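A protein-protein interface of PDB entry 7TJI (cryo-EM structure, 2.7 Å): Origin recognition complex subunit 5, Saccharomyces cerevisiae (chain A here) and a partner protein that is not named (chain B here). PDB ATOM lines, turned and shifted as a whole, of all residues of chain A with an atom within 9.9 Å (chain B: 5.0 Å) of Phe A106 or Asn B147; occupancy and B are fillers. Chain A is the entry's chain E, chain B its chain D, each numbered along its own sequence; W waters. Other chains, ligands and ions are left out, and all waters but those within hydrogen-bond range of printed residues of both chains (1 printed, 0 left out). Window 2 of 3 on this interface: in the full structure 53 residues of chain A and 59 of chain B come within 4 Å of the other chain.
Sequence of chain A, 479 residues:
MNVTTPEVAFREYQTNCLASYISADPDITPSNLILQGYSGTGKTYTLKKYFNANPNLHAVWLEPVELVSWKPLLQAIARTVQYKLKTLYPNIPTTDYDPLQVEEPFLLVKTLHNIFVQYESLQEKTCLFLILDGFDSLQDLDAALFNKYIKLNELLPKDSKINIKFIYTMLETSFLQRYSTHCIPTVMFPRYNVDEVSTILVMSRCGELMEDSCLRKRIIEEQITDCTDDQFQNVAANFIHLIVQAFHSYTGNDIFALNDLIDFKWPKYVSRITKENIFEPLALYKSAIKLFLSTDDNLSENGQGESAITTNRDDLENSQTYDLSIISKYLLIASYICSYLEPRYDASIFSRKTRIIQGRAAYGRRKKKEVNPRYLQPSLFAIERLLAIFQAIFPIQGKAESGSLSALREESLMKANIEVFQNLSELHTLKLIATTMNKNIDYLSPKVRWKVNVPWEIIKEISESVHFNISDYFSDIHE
The side-chain amide nitrogen (ND2) of Asn A114 is in hydrogen-bond range of the backbone carbonyl oxygen (O) of Lys A110 (3.2 Å).
Among the printed residues, pairs that only touch across the chains: Phe A106 with Ile B139 (3.9 Å), Phe A106 with His B140 (3.97 Å), Phe A106 with Thr B144 (3.2 Å), Phe A106 with Asn B147 (3.6 Å), Lys A110 with Thr B151 (3.8 Å), Lys A148 with Ile B139 (3.9 Å) and Leu A155 with Ile B139 (3.8 Å).
Of chain B, only Ile B139, His B140, Thr B144 and Asn B147 come within 4 Å of Phe A106. Of chain A, only Phe A106 comes within 4 Å of Asn B147. Of the printed residues of chain A, Thr B144 touches Phe A106 (3.2 Å). No residue of chain A comes within 4 Å of Ala B145. No residue of chain A comes within 4 Å of Ile B146. No residue of chain A comes within 4 Å of Ala B150. Of the printed residues of chain A, His B140 touches Phe A106 (3.97 Å). Of the printed residues of chain B, Lys A110 touches Thr B151 (3.8 Å). Of the printed residues of chain A, Thr B151 touches Lys A110. Tyr A149 touches none of the printed residues of chain B.
Printed residues of chain A that touch a printed residue of chain B: Phe A106, Lys A110, Lys A148 and Leu A155. Among the printed residues, no Asp or Glu carboxylate lies within 4 Å of a Lys or Arg side-chain nitrogen of the other chain.
Water W1 lies within hydrogen-bond range of the backbone carbonyl oxygen (O) of Ile B139 (2.9 Å), the backbone NH (N) of Phe A106 (3.1 Å) and the side-chain carboxylate (OE1) of Glu A104 (3.3 Å).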
ATOM      1  N   TRP A  70     -10.301 -37.808 -10.875  1.00  0.00           N
ATOM      2  CA  TRP A  70     -10.452 -36.407 -10.397  1.00  0.00           C
ATOM      3  C   TRP A  70     -10.040 -35.386 -11.462  1.00  0.00           C
ATOM      4  O   TRP A  70     -10.724 -34.363 -11.577  1.00  0.00           O
ATOM      5  CB  TRP A  70      -9.651 -36.228  -9.101  1.00  0.00           C
ATOM      6  CG  TRP A  70      -8.168 -36.369  -9.249  1.00  0.00           C
ATOM      7  CD1 TRP A  70      -7.424 -37.492  -9.038  1.00  0.00           C
ATOM      8  CD2 TRP A  70      -7.238 -35.339  -9.623  1.00  0.00           C
ATOM      9  NE1 TRP A  70      -6.099 -37.236  -9.264  1.00  0.00           N
ATOM     10  CE2 TRP A  70      -5.954 -35.924  -9.627  1.00  0.00           C
ATOM     11  CE3 TRP A  70      -7.362 -33.987  -9.963  1.00  0.00           C
ATOM     12  CZ2 TRP A  70      -4.810 -35.201  -9.957  1.00  0.00           C
ATOM     13  CZ3 TRP A  70      -6.230 -33.275 -10.288  1.00  0.00           C
ATOM     14  CH2 TRP A  70      -4.972 -33.876 -10.285  1.00  0.00           C
ATOM     15  N   LEU A  74     -12.341 -32.367 -13.114  1.00  0.00           N
ATOM     16  CA  LEU A  74     -12.011 -30.942 -13.139  1.00  0.00           C
ATOM     17  C   LEU A  74     -12.079 -30.375 -14.554  1.00  0.00           C
ATOM     18  O   LEU A  74     -12.637 -29.286 -14.773  1.00  0.00           O
ATOM     19  CB  LEU A  74     -10.618 -30.708 -12.561  1.00  0.00           C
ATOM     20  CG  LEU A  74     -10.258 -31.103 -11.132  1.00  0.00           C
ATOM     21  CD1 LEU A  74      -8.771 -30.910 -10.911  1.00  0.00           C
ATOM     22  CD2 LEU A  74     -11.059 -30.317 -10.116  1.00  0.00           C
ATOM     23  N   GLN A 101      -6.050 -27.332 -19.871  1.00  0.00           N
ATOM     24  CA  GLN A 101      -5.115 -26.569 -19.057  1.00  0.00           C
ATOM     25  C   GLN A 101      -5.290 -26.845 -17.568  1.00  0.00           C
ATOM     26  O   GLN A 101      -4.334 -26.682 -16.805  1.00  0.00           O
ATOM     27  CB  GLN A 101      -5.289 -25.076 -19.339  1.00  0.00           C
ATOM     28  CG  GLN A 101      -4.008 -24.289 -19.377  1.00  0.00           C
ATOM     29  CD  GLN A 101      -3.386 -24.239 -20.757  1.00  0.00           C
ATOM     30  OE1 GLN A 101      -4.084 -24.288 -21.771  1.00  0.00           O
ATOM     31  NE2 GLN A 101      -2.064 -24.134 -20.803  1.00  0.00           N
ATOM     32  N   VAL A 102      -6.481 -27.259 -17.146  1.00  0.00           N
ATOM     33  CA  VAL A 102      -6.759 -27.558 -15.745  1.00  0.00           C
ATOM     34  C   VAL A 102      -6.167 -28.924 -15.417  1.00  0.00           C
ATOM     35  O   VAL A 102      -6.666 -29.951 -15.880  1.00  0.00           O
ATOM     36  CB  VAL A 102      -8.265 -27.525 -15.457  1.00  0.00           C
ATOM     37  CG1 VAL A 102      -8.547 -27.901 -14.010  1.00  0.00           C
ATOM     38  CG2 VAL A 102      -8.837 -26.158 -15.780  1.00  0.00           C
ATOM     39  N   GLU A 103      -5.096 -28.941 -14.624  1.00  0.00           N
ATOM     40  CA  GLU A 103      -4.504 -30.189 -14.161  1.00  0.00           C
ATOM     41  C   GLU A 103      -4.520 -30.339 -12.645  1.00  0.00           C
ATOM     42  O   GLU A 103      -4.338 -31.456 -12.152  1.00  0.00           O
ATOM     43  CB  GLU A 103      -3.059 -30.327 -14.682  1.00  0.00           C
ATOM     44  CG  GLU A 103      -1.968 -29.866 -13.716  1.00  0.00           C
ATOM     45  CD  GLU A 103      -0.676 -29.482 -14.407  1.00  0.00           C
ATOM     46  OE1 GLU A 103      -0.673 -28.469 -15.134  1.00  0.00           O
ATOM     47  OE2 GLU A 103       0.341 -30.182 -14.212  1.00  0.00           O
ATOM     48  N   GLU A 104      -4.758 -29.268 -11.904  1.00  0.00           N
ATOM     49  CA  GLU A 104      -4.783 -29.231 -10.451  1.00  0.00           C
ATOM     50  C   GLU A 104      -6.037 -28.483 -10.021  1.00  0.00           C
ATOM     51  O   GLU A 104      -6.656 -27.794 -10.838  1.00  0.00           O
ATOM     52  CB  GLU A 104      -3.518 -28.543  -9.911  1.00  0.00           C
ATOM     53  CG  GLU A 104      -2.262 -29.400  -9.992  1.00  0.00           C
ATOM     54  CD  GLU A 104      -2.227 -30.505  -8.951  1.00  0.00           C
ATOM     55  OE1 GLU A 104      -2.245 -30.188  -7.742  1.00  0.00           O
ATOM     56  OE2 GLU A 104      -2.178 -31.690  -9.340  1.00  0.00           O
ATOM     57  N   PRO A 105      -6.484 -28.657  -8.764  1.00  0.00           N
ATOM     58  CA  PRO A 105      -7.655 -27.886  -8.289  1.00  0.00           C
ATOM     59  C   PRO A 105      -7.482 -26.372  -8.303  1.00  0.00           C
ATOM     60  O   PRO A 105      -8.449 -25.643  -8.579  1.00  0.00           O
ATOM     61  CB  PRO A 105      -7.854 -28.411  -6.861  1.00  0.00           C
ATOM     62  CG  PRO A 105      -7.298 -29.767  -6.882  1.00  0.00           C
ATOM     63  CD  PRO A 105      -6.183 -29.789  -7.865  1.00  0.00           C
ATOM     64  N   PHE A 106      -6.275 -25.875  -8.020  1.00  0.00           N
ATOM     65  CA  PHE A 106      -6.067 -24.432  -8.045  1.00  0.00           C
ATOM     66  C   PHE A 106      -6.093 -23.902  -9.472  1.00  0.00           C
ATOM     67  O   PHE A 106      -6.470 -22.746  -9.697  1.00  0.00           O
ATOM     68  CB  PHE A 106      -4.758 -24.061  -7.331  1.00  0.00           C
ATOM     69  CG  PHE A 106      -3.566 -23.936  -8.239  1.00  0.00           C
ATOM     70  CD1 PHE A 106      -2.943 -25.056  -8.766  1.00  0.00           C
ATOM     71  CD2 PHE A 106      -3.059 -22.681  -8.552  1.00  0.00           C
ATOM     72  CE1 PHE A 106      -1.847 -24.925  -9.599  1.00  0.00           C
ATOM     73  CE2 PHE A 106      -1.970 -22.549  -9.385  1.00  0.00           C
ATOM     74  CZ  PHE A 106      -1.361 -23.671  -9.905  1.00  0.00           C
ATOM     75  N   LEU A 107      -5.739 -24.744 -10.444  1.00  0.00           N
ATOM     76  CA  LEU A 107      -5.910 -24.379 -11.842  1.00  0.00           C
ATOM     77  C   LEU A 107      -7.381 -24.277 -12.214  1.00  0.00           C
ATOM     78  O   LEU A 107      -7.747 -23.426 -13.027  1.00  0.00           O
ATOM     79  CB  LEU A 107      -5.192 -25.382 -12.743  1.00  0.00           C
ATOM     80  CG  LEU A 107      -3.667 -25.295 -12.697  1.00  0.00           C
ATOM     81  CD1 LEU A 107      -3.036 -26.316 -13.616  1.00  0.00           C
ATOM     82  CD2 LEU A 107      -3.195 -23.897 -13.041  1.00  0.00           C
ATOM     83  N   LEU A 108      -8.234 -25.119 -11.619  1.00  0.00           N
ATOM     84  CA  LEU A 108      -9.673 -24.973 -11.816  1.00  0.00           C
ATOM     85  C   LEU A 108     -10.184 -23.675 -11.207  1.00  0.00           C
ATOM     86  O   LEU A 108     -11.030 -23.002 -11.806  1.00  0.00           O
ATOM     87  CB  LEU A 108     -10.426 -26.167 -11.223  1.00  0.00           C
ATOM     88  CG  LEU A 108     -11.956 -26.083 -11.345  1.00  0.00           C
ATOM     89  CD1 LEU A 108     -12.418 -26.328 -12.778  1.00  0.00           C
ATOM     90  CD2 LEU A 108     -12.675 -26.992 -10.371  1.00  0.00           C
ATOM     91  N   VAL A 109      -9.671 -23.305 -10.027  1.00  0.00           N
ATOM     92  CA  VAL A 109     -10.057 -22.039  -9.398  1.00  0.00           C
ATOM     93  C   VAL A 109      -9.655 -20.855 -10.278  1.00  0.00           C
ATOM     94  O   VAL A 109     -10.459 -19.949 -10.536  1.00  0.00           O
ATOM     95  CB  VAL A 109      -9.452 -21.940  -7.984  1.00  0.00           C
ATOM     96  CG1 VAL A 109      -9.451 -20.499  -7.472  1.00  0.00           C
ATOM     97  CG2 VAL A 109     -10.208 -22.828  -7.027  1.00  0.00           C
ATOM     98  N   LYS A 110      -8.428 -20.895 -10.809  1.00  0.00           N
ATOM     99  CA  LYS A 110      -7.930 -19.844 -11.696  1.00  0.00           C
ATOM    100  C   LYS A 110      -8.723 -19.765 -13.002  1.00  0.00           C
ATOM    101  O   LYS A 110      -9.075 -18.670 -13.458  1.00  0.00           O
ATOM    102  CB  LYS A 110      -6.448 -20.088 -11.974  1.00  0.00           C
ATOM    103  CG  LYS A 110      -5.813 -19.165 -12.988  1.00  0.00           C
ATOM    104  CD  LYS A 110      -4.311 -19.144 -12.816  1.00  0.00           C
ATOM    105  CE  LYS A 110      -3.619 -20.012 -13.844  1.00  0.00           C
ATOM    106  NZ  LYS A 110      -3.432 -19.289 -15.127  1.00  0.00           N
ATOM    107  N   THR A 111      -9.036 -20.920 -13.600  1.00  0.00           N
ATOM    108  CA  THR A 111      -9.772 -20.944 -14.861  1.00  0.00           C
ATOM    109  C   THR A 111     -11.215 -20.491 -14.679  1.00  0.00           C
ATOM    110  O   THR A 111     -11.747 -19.760 -15.522  1.00  0.00           O
ATOM    111  CB  THR A 111      -9.717 -22.347 -15.467  1.00  0.00           C
ATOM    112  OG1 THR A 111      -8.363 -22.808 -15.470  1.00  0.00           O
ATOM    113  CG2 THR A 111     -10.237 -22.345 -16.892  1.00  0.00           C
ATOM    114  N   LEU A 112     -11.863 -20.900 -13.582  1.00  0.00           N
ATOM    115  CA  LEU A 112     -13.224 -20.450 -13.306  1.00  0.00           C
ATOM    116  C   LEU A 112     -13.265 -18.956 -13.019  1.00  0.00           C
ATOM    117  O   LEU A 112     -14.212 -18.277 -13.422  1.00  0.00           O
ATOM    118  CB  LEU A 112     -13.818 -21.232 -12.136  1.00  0.00           C
ATOM    119  CG  LEU A 112     -14.293 -22.660 -12.396  1.00  0.00           C
ATOM    120  CD1 LEU A 112     -14.760 -23.296 -11.105  1.00  0.00           C
ATOM    121  CD2 LEU A 112     -15.392 -22.704 -13.448  1.00  0.00           C
ATOM    122  N   HIS A 113     -12.240 -18.430 -12.337  1.00  0.00           N
ATOM    123  CA  HIS A 113     -12.127 -16.987 -12.134  1.00  0.00           C
ATOM    124  C   HIS A 113     -11.990 -16.248 -13.460  1.00  0.00           C
ATOM    125  O   HIS A 113     -12.658 -15.226 -13.681  1.00  0.00           O
ATOM    126  CB  HIS A 113     -10.934 -16.696 -11.220  1.00  0.00           C
ATOM    127  CG  HIS A 113     -10.698 -15.242 -10.949  1.00  0.00           C
ATOM    128  ND1 HIS A 113     -11.111 -14.627  -9.788  1.00  0.00           N
ATOM    129  CD2 HIS A 113     -10.056 -14.290 -11.667  1.00  0.00           C
ATOM    130  CE1 HIS A 113     -10.756 -13.356  -9.813  1.00  0.00           C
ATOM    131  NE2 HIS A 113     -10.114 -13.125 -10.943  1.00  0.00           N
ATOM    132  N   ASN A 114     -11.143 -16.764 -14.359  1.00  0.00           N
ATOM    133  CA  ASN A 114     -10.932 -16.132 -15.659  1.00  0.00           C
ATOM    134  C   ASN A 114     -12.188 -16.185 -16.522  1.00  0.00           C
ATOM    135  O   ASN A 114     -12.459 -15.253 -17.288  1.00  0.00           O
ATOM    136  CB  ASN A 114      -9.761 -16.797 -16.379  1.00  0.00           C
ATOM    137  CG  ASN A 114      -8.420 -16.377 -15.820  1.00  0.00           C
ATOM    138  OD1 ASN A 114      -8.248 -15.244 -15.382  1.00  0.00           O
ATOM    139  ND2 ASN A 114      -7.461 -17.293 -15.828  1.00  0.00           N
ATOM    140  N   LYS A 148     -12.246 -30.650  -1.151  1.00  0.00           N
ATOM    141  CA  LYS A 148     -11.904 -29.641  -2.149  1.00  0.00           C
ATOM    142  C   LYS A 148     -13.154 -29.025  -2.764  1.00  0.00           C
ATOM    143  O   LYS A 148     -13.235 -27.803  -2.938  1.00  0.00           O
ATOM    144  CB  LYS A 148     -11.036 -30.260  -3.243  1.00  0.00           C
ATOM    145  CG  LYS A 148      -9.769 -30.921  -2.757  1.00  0.00           C
ATOM    146  CD  LYS A 148      -8.965 -31.450  -3.930  1.00  0.00           C
ATOM    147  CE  LYS A 148      -7.646 -32.039  -3.484  1.00  0.00           C
ATOM    148  NZ  LYS A 148      -7.842 -33.235  -2.637  1.00  0.00           N
ATOM    149  N   TYR A 149     -14.153 -29.852  -3.061  1.00  0.00           N
ATOM    150  CA  TYR A 149     -15.383 -29.336  -3.645  1.00  0.00           C
ATOM    151  C   TYR A 149     -16.241 -28.613  -2.618  1.00  0.00           C
ATOM    152  O   TYR A 149     -17.018 -27.726  -2.991  1.00  0.00           O
ATOM    153  CB  TYR A 149     -16.158 -30.471  -4.307  1.00  0.00           C
ATOM    154  CG  TYR A 149     -15.510 -30.918  -5.581  1.00  0.00           C
ATOM    155  CD1 TYR A 149     -15.830 -30.314  -6.789  1.00  0.00           C
ATOM    156  CD2 TYR A 149     -14.553 -31.924  -5.578  1.00  0.00           C
ATOM    157  CE1 TYR A 149     -15.224 -30.711  -7.957  1.00  0.00           C
ATOM    158  CE2 TYR A 149     -13.944 -32.326  -6.741  1.00  0.00           C
ATOM    159  CZ  TYR A 149     -14.283 -31.714  -7.928  1.00  0.00           C
ATOM    160  OH  TYR A 149     -13.682 -32.110  -9.094  1.00  0.00           O
ATOM    161  N   LEU A 152     -14.386 -25.138  -2.412  1.00  0.00           N
ATOM    162  CA  LEU A 152     -14.114 -24.461  -3.682  1.00  0.00           C
ATOM    163  C   LEU A 152     -14.769 -23.085  -3.797  1.00  0.00           C
ATOM    164  O   LEU A 152     -14.190 -22.185  -4.415  1.00  0.00           O
ATOM    165  CB  LEU A 152     -14.565 -25.333  -4.852  1.00  0.00           C
ATOM    166  CG  LEU A 152     -13.919 -24.980  -6.191  1.00  0.00           C
ATOM    167  CD1 LEU A 152     -12.595 -25.707  -6.349  1.00  0.00           C
ATOM    168  CD2 LEU A 152     -14.849 -25.275  -7.356  1.00  0.00           C
ATOM    169  N   LEU A 155     -12.814 -19.807  -2.692  1.00  0.00           N
ATOM    170  CA  LEU A 155     -11.688 -19.302  -3.461  1.00  0.00           C
ATOM    171  C   LEU A 155     -12.102 -18.485  -4.678  1.00  0.00           C
ATOM    172  O   LEU A 155     -11.262 -17.773  -5.236  1.00  0.00           O
ATOM    173  CB  LEU A 155     -10.787 -20.461  -3.899  1.00  0.00           C
ATOM    174  CG  LEU A 155     -10.146 -21.260  -2.762  1.00  0.00           C
ATOM    175  CD1 LEU A 155      -9.168 -22.277  -3.311  1.00  0.00           C
ATOM    176  CD2 LEU A 155      -9.461 -20.337  -1.769  1.00  0.00           C
ATOM    177  N   LEU A 156     -13.356 -18.561  -5.094  1.00  0.00           N
ATOM    178  CA  LEU A 156     -13.961 -17.802  -6.179  1.00  0.00           C
ATOM    179  C   LEU A 156     -14.384 -16.416  -5.690  1.00  0.00           C
ATOM    180  O   LEU A 156     -14.609 -16.228  -4.491  1.00  0.00           O
ATOM    181  CB  LEU A 156     -15.157 -18.566  -6.741  1.00  0.00           C
ATOM    182  CG  LEU A 156     -14.664 -19.800  -7.500  1.00  0.00           C
ATOM    183  CD1 LEU A 156     -15.769 -20.796  -7.724  1.00  0.00           C
ATOM    184  CD2 LEU A 156     -14.025 -19.403  -8.820  1.00  0.00           C
ATOM    185  N   ILE B 139      -7.038 -27.523  -1.191  1.00  0.00           N
ATOM    186  CA  ILE B 139      -6.846 -27.213  -2.605  1.00  0.00           C
ATOM    187  C   ILE B 139      -5.361 -27.053  -2.926  1.00  0.00           C
ATOM    188  O   ILE B 139      -4.876 -27.564  -3.942  1.00  0.00           O
ATOM    189  CB  ILE B 139      -7.677 -25.971  -2.993  1.00  0.00           C
ATOM    190  CG1 ILE B 139      -9.169 -26.317  -3.073  1.00  0.00           C
ATOM    191  CG2 ILE B 139      -7.233 -25.377  -4.324  1.00  0.00           C
ATOM    192  CD1 ILE B 139      -9.981 -25.973  -1.848  1.00  0.00           C
ATOM    193  N   HIS B 140      -4.607 -26.395  -2.053  1.00  0.00           N
ATOM    194  CA  HIS B 140      -3.218 -26.055  -2.338  1.00  0.00           C
ATOM    195  C   HIS B 140      -2.257 -27.072  -1.738  1.00  0.00           C
ATOM    196  O   HIS B 140      -2.399 -27.465  -0.575  1.00  0.00           O
ATOM    197  CB  HIS B 140      -2.877 -24.657  -1.826  1.00  0.00           C
ATOM    198  CG  HIS B 140      -3.587 -23.562  -2.554  1.00  0.00           C
ATOM    199  ND1 HIS B 140      -4.678 -22.906  -2.030  1.00  0.00           N
ATOM    200  CD2 HIS B 140      -3.366 -23.009  -3.770  1.00  0.00           C
ATOM    201  CE1 HIS B 140      -5.094 -21.993  -2.886  1.00  0.00           C
ATOM    202  NE2 HIS B 140      -4.314 -22.034  -3.950  1.00  0.00           N
ATOM    203  N   GLN B 143       3.933 -27.251  -3.502  1.00  0.00           N
ATOM    204  CA  GLN B 143       4.401 -26.601  -4.719  1.00  0.00           C
ATOM    205  C   GLN B 143       3.352 -25.687  -5.333  1.00  0.00           C
ATOM    206  O   GLN B 143       3.700 -24.642  -5.893  1.00  0.00           O
ATOM    207  CB  GLN B 143       4.830 -27.654  -5.753  1.00  0.00           C
ATOM    208  CG  GLN B 143       3.783 -28.662  -6.363  1.00  0.00           C
ATOM    209  CD  GLN B 143       4.239 -29.718  -7.407  1.00  0.00           C
ATOM    210  OE1 GLN B 143       5.412 -30.071  -7.546  1.00  0.00           O
ATOM    211  NE2 GLN B 143       3.261 -30.227  -8.144  1.00  0.00           N
ATOM    212  N   THR B 144       2.079 -26.056  -5.227  1.00  0.00           N
ATOM    213  CA  THR B 144       1.008 -25.328  -5.893  1.00  0.00           C
ATOM    214  C   THR B 144       0.662 -24.023  -5.165  1.00  0.00           C
ATOM    215  O   THR B 144       0.209 -23.063  -5.803  1.00  0.00           O
ATOM    216  CB  THR B 144      -0.183 -26.291  -6.052  1.00  0.00           C
ATOM    217  OG1 THR B 144      -0.323 -26.658  -7.430  1.00  0.00           O
ATOM    218  CG2 THR B 144      -1.492 -25.740  -5.543  1.00  0.00           C
ATOM    219  N   ALA B 145       0.948 -23.946  -3.860  1.00  0.00           N
ATOM    220  CA  ALA B 145       0.687 -22.728  -3.094  1.00  0.00           C
ATOM    221  C   ALA B 145       1.563 -21.564  -3.543  1.00  0.00           C
ATOM    222  O   ALA B 145       1.142 -20.412  -3.432  1.00  0.00           O
ATOM    223  CB  ALA B 145       0.887 -22.980  -1.601  1.00  0.00           C
ATOM    224  N   ILE B 146       2.761 -21.843  -4.063  1.00  0.00           N
ATOM    225  CA  ILE B 146       3.622 -20.791  -4.599  1.00  0.00           C
ATOM    226  C   ILE B 146       2.983 -20.147  -5.827  1.00  0.00           C
ATOM    227  O   ILE B 146       2.913 -18.915  -5.941  1.00  0.00           O
ATOM    228  CB  ILE B 146       5.014 -21.366  -4.921  1.00  0.00           C
ATOM    229  CG1 ILE B 146       5.625 -21.995  -3.668  1.00  0.00           C
ATOM    230  CG2 ILE B 146       5.929 -20.294  -5.496  1.00  0.00           C
ATOM    231  CD1 ILE B 146       6.647 -23.062  -3.962  1.00  0.00           C
ATOM    232  N   ASN B 147       2.480 -20.978  -6.747  1.00  0.00           N
ATOM    233  CA  ASN B 147       1.788 -20.475  -7.929  1.00  0.00           C
ATOM    234  C   ASN B 147       0.497 -19.757  -7.558  1.00  0.00           C
ATOM    235  O   ASN B 147       0.153 -18.741  -8.170  1.00  0.00           O
ATOM    236  CB  ASN B 147       1.497 -21.621  -8.897  1.00  0.00           C
ATOM    237  CG  ASN B 147       2.725 -22.070  -9.651  1.00  0.00           C
ATOM    238  OD1 ASN B 147       3.512 -21.254 -10.124  1.00  0.00           O
ATOM    239  ND2 ASN B 147       2.898 -23.379  -9.765  1.00  0.00           N
ATOM    240  N   GLY B 148      -0.218 -20.267  -6.549  1.00  0.00           N
ATOM    241  CA  GLY B 148      -1.429 -19.602  -6.090  1.00  0.00           C
ATOM    242  C   GLY B 148      -1.170 -18.238  -5.477  1.00  0.00           C
ATOM    243  O   GLY B 148      -1.900 -17.280  -5.752  1.00  0.00           O
ATOM    244  N   ILE B 149      -0.111 -18.131  -4.660  1.00  0.00           N
ATOM    245  CA  ILE B 149       0.291 -16.851  -4.080  1.00  0.00           C
ATOM    246  C   ILE B 149       0.679 -15.869  -5.177  1.00  0.00           C
ATOM    247  O   ILE B 149       0.272 -14.702  -5.150  1.00  0.00           O
ATOM    248  CB  ILE B 149       1.435 -17.059  -3.063  1.00  0.00           C
ATOM    249  CG1 ILE B 149       0.909 -17.639  -1.753  1.00  0.00           C
ATOM    250  CG2 ILE B 149       2.173 -15.757  -2.754  1.00  0.00           C
ATOM    251  CD1 ILE B 149       1.994 -18.216  -0.881  1.00  0.00           C
ATOM    252  N   ALA B 150       1.422 -16.340  -6.187  1.00  0.00           N
ATOM    253  CA  ALA B 150       1.862 -15.458  -7.268  1.00  0.00           C
ATOM    254  C   ALA B 150       0.697 -14.963  -8.124  1.00  0.00           C
ATOM    255  O   ALA B 150       0.626 -13.767  -8.448  1.00  0.00           O
ATOM    256  CB  ALA B 150       2.891 -16.175  -8.135  1.00  0.00           C
ATOM    257  N   THR B 151      -0.234 -15.858  -8.485  1.00  0.00           N
ATOM    258  CA  THR B 151      -1.352 -15.431  -9.319  1.00  0.00           C
ATOM    259  C   THR B 151      -2.315 -14.529  -8.549  1.00  0.00           C
ATOM    260  O   THR B 151      -2.828 -13.554  -9.119  1.00  0.00           O
ATOM    261  CB  THR B 151      -2.074 -16.636  -9.956  1.00  0.00           C
ATOM    262  OG1 THR B 151      -3.061 -16.163 -10.879  1.00  0.00           O
ATOM    263  CG2 THR B 151      -2.764 -17.544  -8.951  1.00  0.00           C
ATOM    264  N   GLN B 152      -2.506 -14.776  -7.243  1.00  0.00           N
ATOM    265  CA  GLN B 152      -3.334 -13.877  -6.455  1.00  0.00           C
ATOM    266  C   GLN B 152      -2.646 -12.541  -6.241  1.00  0.00           C
ATOM    267  O   GLN B 152      -3.319 -11.511  -6.213  1.00  0.00           O
ATOM    268  CB  GLN B 152      -3.694 -14.519  -5.119  1.00  0.00           C
ATOM    269  CG  GLN B 152      -4.765 -15.588  -5.214  1.00  0.00           C
ATOM    270  CD  GLN B 152      -5.033 -16.248  -3.885  1.00  0.00           C
ATOM    271  OE1 GLN B 152      -5.715 -15.689  -3.031  1.00  0.00           O
ATOM    272  NE2 GLN B 152      -4.488 -17.442  -3.696  1.00  0.00           N
ATOM    273  N   LEU B 180       9.007 -22.727 -11.261  1.00  0.00           N
ATOM    274  CA  LEU B 180       8.712 -22.636  -9.833  1.00  0.00           C
ATOM    275  C   LEU B 180       9.849 -21.995  -9.044  1.00  0.00           C
ATOM    276  O   LEU B 180       9.591 -21.248  -8.093  1.00  0.00           O
ATOM    277  CB  LEU B 180       8.398 -24.025  -9.283  1.00  0.00           C
ATOM    278  CG  LEU B 180       7.462 -24.094  -8.075  1.00  0.00           C
ATOM    279  CD1 LEU B 180       6.112 -23.466  -8.395  1.00  0.00           C
ATOM    280  CD2 LEU B 180       7.296 -25.532  -7.622  1.00  0.00           C
ATOM    281  N   VAL B 183       9.556 -18.194  -9.906  1.00  0.00           N
ATOM    282  CA  VAL B 183       8.371 -17.621  -9.274  1.00  0.00           C
ATOM    283  C   VAL B 183       8.583 -17.479  -7.772  1.00  0.00           C
ATOM    284  O   VAL B 183       8.248 -16.445  -7.176  1.00  0.00           O
ATOM    285  CB  VAL B 183       7.136 -18.480  -9.609  1.00  0.00           C
ATOM    286  CG1 VAL B 183       5.978 -18.208  -8.657  1.00  0.00           C
ATOM    287  CG2 VAL B 183       6.707 -18.246 -11.047  1.00  0.00           C
HETATM  288  O   HOH W   1      -3.998 -27.540  -6.737  1.00  0.00           O
